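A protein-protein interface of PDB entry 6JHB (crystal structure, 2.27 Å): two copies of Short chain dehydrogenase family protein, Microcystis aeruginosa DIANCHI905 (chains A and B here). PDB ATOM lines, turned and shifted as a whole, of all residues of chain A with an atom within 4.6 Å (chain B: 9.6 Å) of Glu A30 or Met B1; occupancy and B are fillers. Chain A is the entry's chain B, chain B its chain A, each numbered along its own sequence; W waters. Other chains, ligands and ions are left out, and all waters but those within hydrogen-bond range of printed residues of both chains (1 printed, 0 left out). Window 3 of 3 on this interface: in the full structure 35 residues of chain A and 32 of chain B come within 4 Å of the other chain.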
ATOM      1  N   MET A   1      28.866  -7.665  14.140  1.00  0.00           N
ATOM      2  CA  MET A   1      29.351  -6.282  14.145  1.00  0.00           C
ATOM      3  C   MET A   1      29.260  -5.680  15.552  1.00  0.00           C
ATOM      4  O   MET A   1      28.201  -5.665  16.193  1.00  0.00           O
ATOM      5  CB  MET A   1      28.531  -5.448  13.163  1.00  0.00           C
ATOM      6  CG  MET A   1      29.016  -4.024  12.981  1.00  0.00           C
ATOM      7  SD  MET A   1      27.932  -3.151  11.831  1.00  0.00           S
ATOM      8  CE  MET A   1      28.758  -3.519  10.299  1.00  0.00           C
ATOM      9  N   LEU A   3      28.857  -2.623  17.674  1.00  0.00           N
ATOM     10  CA  LEU A   3      28.245  -1.339  17.463  1.00  0.00           C
ATOM     11  C   LEU A   3      28.803  -0.245  18.379  1.00  0.00           C
ATOM     12  O   LEU A   3      28.524   0.943  18.145  1.00  0.00           O
ATOM     13  CB  LEU A   3      26.727  -1.480  17.583  1.00  0.00           C
ATOM     14  CG  LEU A   3      26.113  -2.318  16.449  1.00  0.00           C
ATOM     15  CD1 LEU A   3      24.597  -2.331  16.506  1.00  0.00           C
ATOM     16  CD2 LEU A   3      26.552  -1.817  15.073  1.00  0.00           C
ATOM     17  N   LEU A   5      28.350   0.247  21.642  1.00  0.00           N
ATOM     18  CA  LEU A   5      27.267   0.793  22.410  1.00  0.00           C
ATOM     19  C   LEU A   5      27.311   0.471  23.887  1.00  0.00           C
ATOM     20  O   LEU A   5      26.521   1.043  24.661  1.00  0.00           O
ATOM     21  CB  LEU A   5      25.954   0.271  21.842  1.00  0.00           C
ATOM     22  CG  LEU A   5      25.507   0.943  20.557  1.00  0.00           C
ATOM     23  CD1 LEU A   5      24.103   0.483  20.238  1.00  0.00           C
ATOM     24  CD2 LEU A   5      25.554   2.453  20.694  1.00  0.00           C
ATOM     25  N   LYS A   6      28.229  -0.413  24.278  1.00  0.00           N
ATOM     26  CA  LYS A   6      28.370  -0.829  25.673  1.00  0.00           C
ATOM     27  C   LYS A   6      28.397   0.386  26.580  1.00  0.00           C
ATOM     28  O   LYS A   6      29.223   1.265  26.394  1.00  0.00           O
ATOM     29  CB  LYS A   6      29.640  -1.675  25.886  1.00  0.00           C
ATOM     30  CG  LYS A   6      29.646  -2.460  27.203  1.00  0.00           C
ATOM     31  N   LYS A  26      16.511  -3.970  21.783  1.00  0.00           N
ATOM     32  CA  LYS A  26      17.679  -4.143  20.957  1.00  0.00           C
ATOM     33  C   LYS A  26      18.848  -3.256  21.430  1.00  0.00           C
ATOM     34  O   LYS A  26      20.020  -3.659  21.348  1.00  0.00           O
ATOM     35  CB  LYS A  26      17.328  -3.872  19.496  1.00  0.00           C
ATOM     36  CG  LYS A  26      18.058  -4.782  18.512  1.00  0.00           C
ATOM     37  CD  LYS A  26      17.076  -5.457  17.555  1.00  0.00           C
ATOM     38  CE  LYS A  26      17.553  -6.835  17.180  1.00  0.00           C
ATOM     39  NZ  LYS A  26      16.399  -7.739  17.030  1.00  0.00           N
ATOM     40  N   LEU A  27      18.551  -2.057  21.917  1.00  0.00           N
ATOM     41  CA  LEU A  27      19.628  -1.224  22.471  1.00  0.00           C
ATOM     42  C   LEU A  27      20.162  -1.872  23.754  1.00  0.00           C
ATOM     43  O   LEU A  27      21.377  -1.942  23.966  1.00  0.00           O
ATOM     44  CB  LEU A  27      19.160   0.192  22.733  1.00  0.00           C
ATOM     45  CG  LEU A  27      18.911   1.055  21.498  1.00  0.00           C
ATOM     46  CD1 LEU A  27      18.192   2.333  21.872  1.00  0.00           C
ATOM     47  CD2 LEU A  27      20.211   1.416  20.795  1.00  0.00           C
ATOM     48  N   ALA A  28      19.252  -2.397  24.577  1.00  0.00           N
ATOM     49  CA  ALA A  28      19.661  -3.121  25.781  1.00  0.00           C
ATOM     50  C   ALA A  28      20.603  -4.248  25.417  1.00  0.00           C
ATOM     51  O   ALA A  28      21.626  -4.434  26.081  1.00  0.00           O
ATOM     52  CB  ALA A  28      18.461  -3.665  26.532  1.00  0.00           C
ATOM     53  N   GLU A  29      20.271  -4.960  24.341  1.00  0.00           N
ATOM     54  CA  GLU A  29      21.026  -6.128  23.903  1.00  0.00           C
ATOM     55  C   GLU A  29      22.405  -5.757  23.439  1.00  0.00           C
ATOM     56  O   GLU A  29      23.310  -6.582  23.535  1.00  0.00           O
ATOM     57  CB  GLU A  29      20.320  -6.875  22.780  1.00  0.00           C
ATOM     58  CG  GLU A  29      20.872  -8.276  22.571  1.00  0.00           C
ATOM     59  CD  GLU A  29      20.051  -9.063  21.576  1.00  0.00           C
ATOM     60  OE1 GLU A  29      19.637 -10.201  21.896  1.00  0.00           O
ATOM     61  OE2 GLU A  29      19.803  -8.527  20.474  1.00  0.00           O
ATOM     62  N   GLU A  30      22.580  -4.530  22.953  1.00  0.00           N
ATOM     63  CA  GLU A  30      23.931  -4.068  22.567  1.00  0.00           C
ATOM     64  C   GLU A  30      24.761  -3.531  23.739  1.00  0.00           C
ATOM     65  O   GLU A  30      25.903  -3.117  23.550  1.00  0.00           O
ATOM     66  CB  GLU A  30      23.856  -2.997  21.477  1.00  0.00           C
ATOM     67  CG  GLU A  30      23.183  -3.468  20.195  1.00  0.00           C
ATOM     68  CD  GLU A  30      23.876  -4.660  19.537  1.00  0.00           C
ATOM     69  OE1 GLU A  30      25.122  -4.652  19.405  1.00  0.00           O
ATOM     70  OE2 GLU A  30      23.171  -5.611  19.140  1.00  0.00           O
ATOM     71  N   GLY A  31      24.178  -3.504  24.933  1.00  0.00           N
ATOM     72  CA  GLY A  31      24.876  -3.016  26.109  1.00  0.00           C
ATOM     73  C   GLY A  31      24.515  -1.624  26.583  1.00  0.00           C
ATOM     74  O   GLY A  31      25.244  -1.067  27.415  1.00  0.00           O
ATOM     75  N   CYS A  32      23.414  -1.053  26.082  1.00  0.00           N
ATOM     76  CA  CYS A  32      22.939   0.272  26.553  1.00  0.00           C
ATOM     77  C   CYS A  32      22.189   0.209  27.857  1.00  0.00           C
ATOM     78  O   CYS A  32      21.463  -0.741  28.113  1.00  0.00           O
ATOM     79  CB  CYS A  32      21.961   0.917  25.565  1.00  0.00           C
ATOM     80  SG  CYS A  32      22.680   1.461  24.021  1.00  0.00           S
ATOM     81  N   ASN A 237      16.450  -2.817  13.976  1.00  0.00           N
ATOM     82  CA  ASN A 237      17.822  -3.055  13.527  1.00  0.00           C
ATOM     83  C   ASN A 237      18.482  -1.830  12.950  1.00  0.00           C
ATOM     84  O   ASN A 237      19.621  -1.502  13.270  1.00  0.00           O
ATOM     85  CB  ASN A 237      17.865  -4.166  12.496  1.00  0.00           C
ATOM     86  CG  ASN A 237      17.716  -5.530  13.122  1.00  0.00           C
ATOM     87  OD1 ASN A 237      18.106  -5.744  14.272  1.00  0.00           O
ATOM     88  ND2 ASN A 237      17.133  -6.460  12.375  1.00  0.00           N
ATOM     89  N   VAL A 240      18.959   0.926  15.605  1.00  0.00           N
ATOM     90  CA  VAL A 240      20.097   0.627  16.473  1.00  0.00           C
ATOM     91  C   VAL A 240      21.422   0.875  15.784  1.00  0.00           C
ATOM     92  O   VAL A 240      22.365   1.358  16.423  1.00  0.00           O
ATOM     93  CB  VAL A 240      19.995  -0.799  17.029  1.00  0.00           C
ATOM     94  CG1 VAL A 240      21.311  -1.291  17.579  1.00  0.00           C
ATOM     95  CG2 VAL A 240      18.947  -0.810  18.132  1.00  0.00           C
ATOM     96  N   MET B   1      26.018  -6.664  17.251  1.00  0.00           N
ATOM     97  CA  MET B   1      24.813  -7.057  16.460  1.00  0.00           C
ATOM     98  C   MET B   1      25.163  -8.232  15.530  1.00  0.00           C
ATOM     99  O   MET B   1      26.114  -8.167  14.768  1.00  0.00           O
ATOM    100  CB  MET B   1      24.307  -5.861  15.659  1.00  0.00           C
ATOM    101  CG  MET B   1      23.056  -6.143  14.836  1.00  0.00           C
ATOM    102  SD  MET B   1      22.387  -4.741  13.917  1.00  0.00           S
ATOM    103  CE  MET B   1      21.327  -4.060  15.185  1.00  0.00           C
ATOM    104  N   ASP B   2      24.394  -9.305  15.616  1.00  0.00           N
ATOM    105  CA  ASP B   2      24.563 -10.450  14.755  1.00  0.00           C
ATOM    106  C   ASP B   2      23.910 -10.192  13.397  1.00  0.00           C
ATOM    107  O   ASP B   2      22.693 -10.099  13.292  1.00  0.00           O
ATOM    108  CB  ASP B   2      23.956 -11.708  15.388  1.00  0.00           C
ATOM    109  CG  ASP B   2      24.262 -12.975  14.572  1.00  0.00           C
ATOM    110  OD1 ASP B   2      24.693 -12.864  13.411  1.00  0.00           O
ATOM    111  OD2 ASP B   2      24.087 -14.090  15.093  1.00  0.00           O
ATOM    112  N   LEU B   3      24.734 -10.139  12.361  1.00  0.00           N
ATOM    113  CA  LEU B   3      24.281  -9.785  11.041  1.00  0.00           C
ATOM    114  C   LEU B   3      23.854 -11.000  10.196  1.00  0.00           C
ATOM    115  O   LEU B   3      23.362 -10.829   9.078  1.00  0.00           O
ATOM    116  CB  LEU B   3      25.384  -8.983  10.333  1.00  0.00           C
ATOM    117  CG  LEU B   3      25.790  -7.651  10.974  1.00  0.00           C
ATOM    118  CD1 LEU B   3      26.651  -6.856  10.023  1.00  0.00           C
ATOM    119  CD2 LEU B   3      24.618  -6.782  11.382  1.00  0.00           C
ATOM    120  N   GLY B   4      24.034 -12.208  10.729  1.00  0.00           N
ATOM    121  CA  GLY B   4      23.542 -13.429  10.074  1.00  0.00           C
ATOM    122  C   GLY B   4      24.291 -13.714   8.769  1.00  0.00           C
ATOM    123  O   GLY B   4      23.730 -14.224   7.814  1.00  0.00           O
ATOM    124  N   LEU B   5      25.565 -13.376   8.728  1.00  0.00           N
ATOM    125  CA  LEU B   5      26.337 -13.441   7.481  1.00  0.00           C
ATOM    126  C   LEU B   5      27.281 -14.620   7.397  1.00  0.00           C
ATOM    127  O   LEU B   5      28.020 -14.753   6.405  1.00  0.00           O
ATOM    128  CB  LEU B   5      27.151 -12.151   7.282  1.00  0.00           C
ATOM    129  CG  LEU B   5      26.388 -10.942   6.761  1.00  0.00           C
ATOM    130  CD1 LEU B   5      27.293  -9.729   6.660  1.00  0.00           C
ATOM    131  CD2 LEU B   5      25.738 -11.252   5.413  1.00  0.00           C
ATOM    132  N   GLU B  29      34.990 -10.189   8.260  1.00  0.00           N
ATOM    133  CA  GLU B  29      34.811 -10.042   9.712  1.00  0.00           C
ATOM    134  C   GLU B  29      33.446 -10.569  10.182  1.00  0.00           C
ATOM    135  O   GLU B  29      33.338 -11.232  11.205  1.00  0.00           O
ATOM    136  CB  GLU B  29      34.982  -8.572  10.105  1.00  0.00           C
ATOM    137  CG  GLU B  29      35.564  -8.357  11.498  1.00  0.00           C
ATOM    138  N   GLU B  30      32.393 -10.292   9.424  1.00  0.00           N
ATOM    139  CA  GLU B  30      31.085 -10.854   9.755  1.00  0.00           C
ATOM    140  C   GLU B  30      30.951 -12.343   9.409  1.00  0.00           C
ATOM    141  O   GLU B  30      29.957 -12.965   9.722  1.00  0.00           O
ATOM    142  CB  GLU B  30      29.997 -10.011   9.110  1.00  0.00           C
ATOM    143  CG  GLU B  30      30.043  -8.576   9.611  1.00  0.00           C
ATOM    144  CD  GLU B  30      30.049  -8.475  11.139  1.00  0.00           C
ATOM    145  OE1 GLU B  30      29.060  -8.885  11.779  1.00  0.00           O
ATOM    146  OE2 GLU B  30      31.038  -7.989  11.711  1.00  0.00           O
ATOM    147  N   ASN B 237      30.790   0.121   7.001  1.00  0.00           N
ATOM    148  CA  ASN B 237      29.872  -0.294   8.022  1.00  0.00           C
ATOM    149  C   ASN B 237      28.439  -0.324   7.492  1.00  0.00           C
ATOM    150  O   ASN B 237      27.709  -1.306   7.691  1.00  0.00           O
ATOM    151  CB  ASN B 237      30.002   0.578   9.255  1.00  0.00           C
ATOM    152  CG  ASN B 237      31.266   0.282  10.069  1.00  0.00           C
ATOM    153  OD1 ASN B 237      31.868  -0.794   9.977  1.00  0.00           O
ATOM    154  ND2 ASN B 237      31.666   1.246  10.873  1.00  0.00           N
ATOM    155  N   VAL B 240      27.863  -3.167   4.661  1.00  0.00           N
ATOM    156  CA  VAL B 240      27.765  -4.449   5.362  1.00  0.00           C
ATOM    157  C   VAL B 240      26.408  -4.611   6.043  1.00  0.00           C
ATOM    158  O   VAL B 240      25.804  -5.691   5.927  1.00  0.00           O
ATOM    159  CB  VAL B 240      28.890  -4.602   6.400  1.00  0.00           C
ATOM    160  CG1 VAL B 240      28.704  -5.850   7.249  1.00  0.00           C
ATOM    161  CG2 VAL B 240      30.225  -4.686   5.688  1.00  0.00           C
ATOM    162  N   PHE B 241      25.904  -3.563   6.718  1.00  0.00           N
ATOM    163  CA  PHE B 241      24.560  -3.659   7.317  1.00  0.00           C
ATOM    164  C   PHE B 241      23.507  -3.888   6.244  1.00  0.00           C
ATOM    165  O   PHE B 241      22.620  -4.696   6.419  1.00  0.00           O
ATOM    166  CB  PHE B 241      24.207  -2.430   8.178  1.00  0.00           C
ATOM    167  CG  PHE B 241      22.776  -2.414   8.655  1.00  0.00           C
ATOM    168  CD1 PHE B 241      22.426  -2.988   9.860  1.00  0.00           C
ATOM    169  CD2 PHE B 241      21.788  -1.828   7.889  1.00  0.00           C
ATOM    170  CE1 PHE B 241      21.110  -2.982  10.297  1.00  0.00           C
ATOM    171  CE2 PHE B 241      20.470  -1.817   8.303  1.00  0.00           C
ATOM    172  CZ  PHE B 241      20.124  -2.393   9.505  1.00  0.00           C
ATOM    173  N   LEU B 242      23.597  -3.188   5.126  1.00  0.00           N
ATOM    174  CA  LEU B 242      22.632  -3.403   4.044  1.00  0.00           C
ATOM    175  C   LEU B 242      22.746  -4.791   3.464  1.00  0.00           C
ATOM    176  O   LEU B 242      21.754  -5.346   2.977  1.00  0.00           O
ATOM    177  CB  LEU B 242      22.831  -2.396   2.926  1.00  0.00           C
ATOM    178  CG  LEU B 242      22.400  -0.970   3.288  1.00  0.00           C
ATOM    179  CD1 LEU B 242      22.872  -0.017   2.197  1.00  0.00           C
ATOM    180  CD2 LEU B 242      20.896  -0.862   3.529  1.00  0.00           C
ATOM    181  N   SER B 244      23.276  -7.458   5.096  1.00  0.00           N
ATOM    182  CA  SER B 244      23.027  -8.424   6.131  1.00  0.00           C
ATOM    183  C   SER B 244      21.570  -8.902   6.206  1.00  0.00           C
ATOM    184  O   SER B 244      20.678  -8.376   5.540  1.00  0.00           O
ATOM    185  CB  SER B 244      23.440  -7.841   7.466  1.00  0.00           C
ATOM    186  OG  SER B 244      22.364  -7.176   8.087  1.00  0.00           O
ATOM    187  N   GLU B 245      21.371  -9.921   7.032  1.00  0.00           N
ATOM    188  CA  GLU B 245      20.046 -10.390   7.419  1.00  0.00           C
ATOM    189  C   GLU B 245      19.238  -9.295   8.154  1.00  0.00           C
ATOM    190  O   GLU B 245      18.000  -9.236   8.033  1.00  0.00           O
ATOM    191  CB  GLU B 245      20.189 -11.620   8.327  1.00  0.00           C
ATOM    192  CG  GLU B 245      18.907 -12.410   8.529  1.00  0.00           C
ATOM    193  CD  GLU B 245      18.344 -12.961   7.229  1.00  0.00           C
ATOM    194  OE1 GLU B 245      19.048 -12.960   6.202  1.00  0.00           O
ATOM    195  OE2 GLU B 245      17.188 -13.406   7.226  1.00  0.00           O
ATOM    196  N   CYS B 246      19.934  -8.406   8.857  1.00  0.00           N
ATOM    197  CA  CYS B 246      19.259  -7.377   9.660  1.00  0.00           C
ATOM    198  C   CYS B 246      18.553  -6.349   8.812  1.00  0.00           C
ATOM    199  O   CYS B 246      17.659  -5.640   9.287  1.00  0.00           O
ATOM    200  CB  CYS B 246      20.235  -6.670  10.581  1.00  0.00           C
ATOM    201  SG  CYS B 246      20.885  -7.814  11.808  1.00  0.00           S
ATOM    202  N   ALA B 247      18.938  -6.281   7.550  1.00  0.00           N
ATOM    203  CA  ALA B 247      18.346  -5.332   6.643  1.00  0.00           C
ATOM    204  C   ALA B 247      17.220  -5.950   5.820  1.00  0.00           C
ATOM    205  O   ALA B 247      16.909  -5.470   4.730  1.00  0.00           O
ATOM    206  CB  ALA B 247      19.430  -4.775   5.755  1.00  0.00           C
HETATM  207  O   HOH W   1      27.445 -10.548  12.835  1.00  0.00           O
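Water W1 lies within hydrogen-bond range of the side-chain carboxylate (OE1) of Glu B30 (2.5 Å), the backbone NH (N) of Leu B3 (2.8 Å), the backbone carbonyl oxygen (O) of Met B1 (3.3 Å) and the backbone NH (N) of Met A1 (3.5 Å).
No residue of chain B comes within 4 Å of Ala A28.
Glu A30 touches just one residue of chain B: Met B1 (3.1 Å).
No residue of chain B comes within 4 Å of Gly A31.
Printed residues of chain B within 4 Å of Asn A237: Met B1 (3.6 Å), Phe B241 (3.6 Å) and Cys B246 (3.2 Å).
Met B1 touches just these residues of chain A: Met A1, Leu A3, Glu A30, Asn A237 and Val A240.
Printed residues of chain A within 4 Å of Val B240: Met A1.
The nearest residue of chain B that does not touch Glu A30 is Asp B2 (5.2 Å).
The nearest printed residue of chain A that does not touch Met B1 is Lys A26 (4.7 Å).
Among the printed residues, merely in contact across the chains: Met A1 with Leu B3 (3.9 Å), Met A1 with Asn B237 (3.6 Å), Met A1 with Val B240 (3.8 Å), Leu A3 with Met B1 (3.6 Å), Asn A237 with Met B1 (3.6 Å), Asn A237 with Phe B241 (3.6 Å) and Val A240 with Met B1 (3.7 Å).
Met A1 touches Leu B3, and with the chains exchanged Leu A3 touches Met B1.
Met A1 touches Glu B30, and with the chains exchanged Glu A30 touches Met B1.
Met A1 touches Asn B237, and with the chains exchanged Asn A237 touches Met B1.
Met A1 touches Val B240, and with the chains exchanged Val A240 touches Met B1.
Positions printed for both chains: 1, 3, 5, 29, 30, 237 and 240.
Of the 11 pairs that touch across the chains among the printed residues, 9 have their exchanged pair printed and touching as well.
Of the 13 printed residues of chain A, 5 touch a printed residue of chain B.
Printed residues of chain A that touch a printed residue of chain B: Met A1, Leu A3, Glu A30, Asn A237 and Val A240.
Of the 15 printed residues of chain B, 7 touch a printed residue of chain A.
Printed residues of chain B that touch a printed residue of chain A: Met B1, Leu B3, Glu B30, Asn B237, Val B240, Phe B241 and Cys B246.
Hydrophobic or aromatic side chains of chain B that line the printed part of chain A: Met B1, Leu B3, Val B240 and Phe B241.
Along chain B the printed residues that touch a printed residue of chain A span positions 1 to 246.
Among the printed residues, 11 pairs touch across the chains.
SG of Cys B246 sits at hydrogen-bond distance from O of Asp B2 (3.3 Å).
N of Glu B245 sits at hydrogen-bond distance from O of Leu B3.
The side-chain hydroxyl of Ser B244 sits at hydrogen-bond distance from the backbone carbonyl oxygen of Phe B241, 3.0 Å away.
The side-chain hydroxyl (OG) of Ser B244 sits at hydrogen-bond distance from the backbone NH (N) of Cys B246 (2.8 Å).
O of Met A1 is in hydrogen-bond range of N of Met B1, 2.6 Å away.
The backbone NH (N) of Met B1 is in hydrogen-bond range of the side-chain carboxylate (OE1) of Glu A30.
The backbone NH (N) of Met A1 lies within hydrogen-bond range of the side-chain carboxylate (OE1) of Glu B30, at 2.7 Å.
ND2 of Asn A237 sits at hydrogen-bond distance from O of Cys B246, at 3.2 Å.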
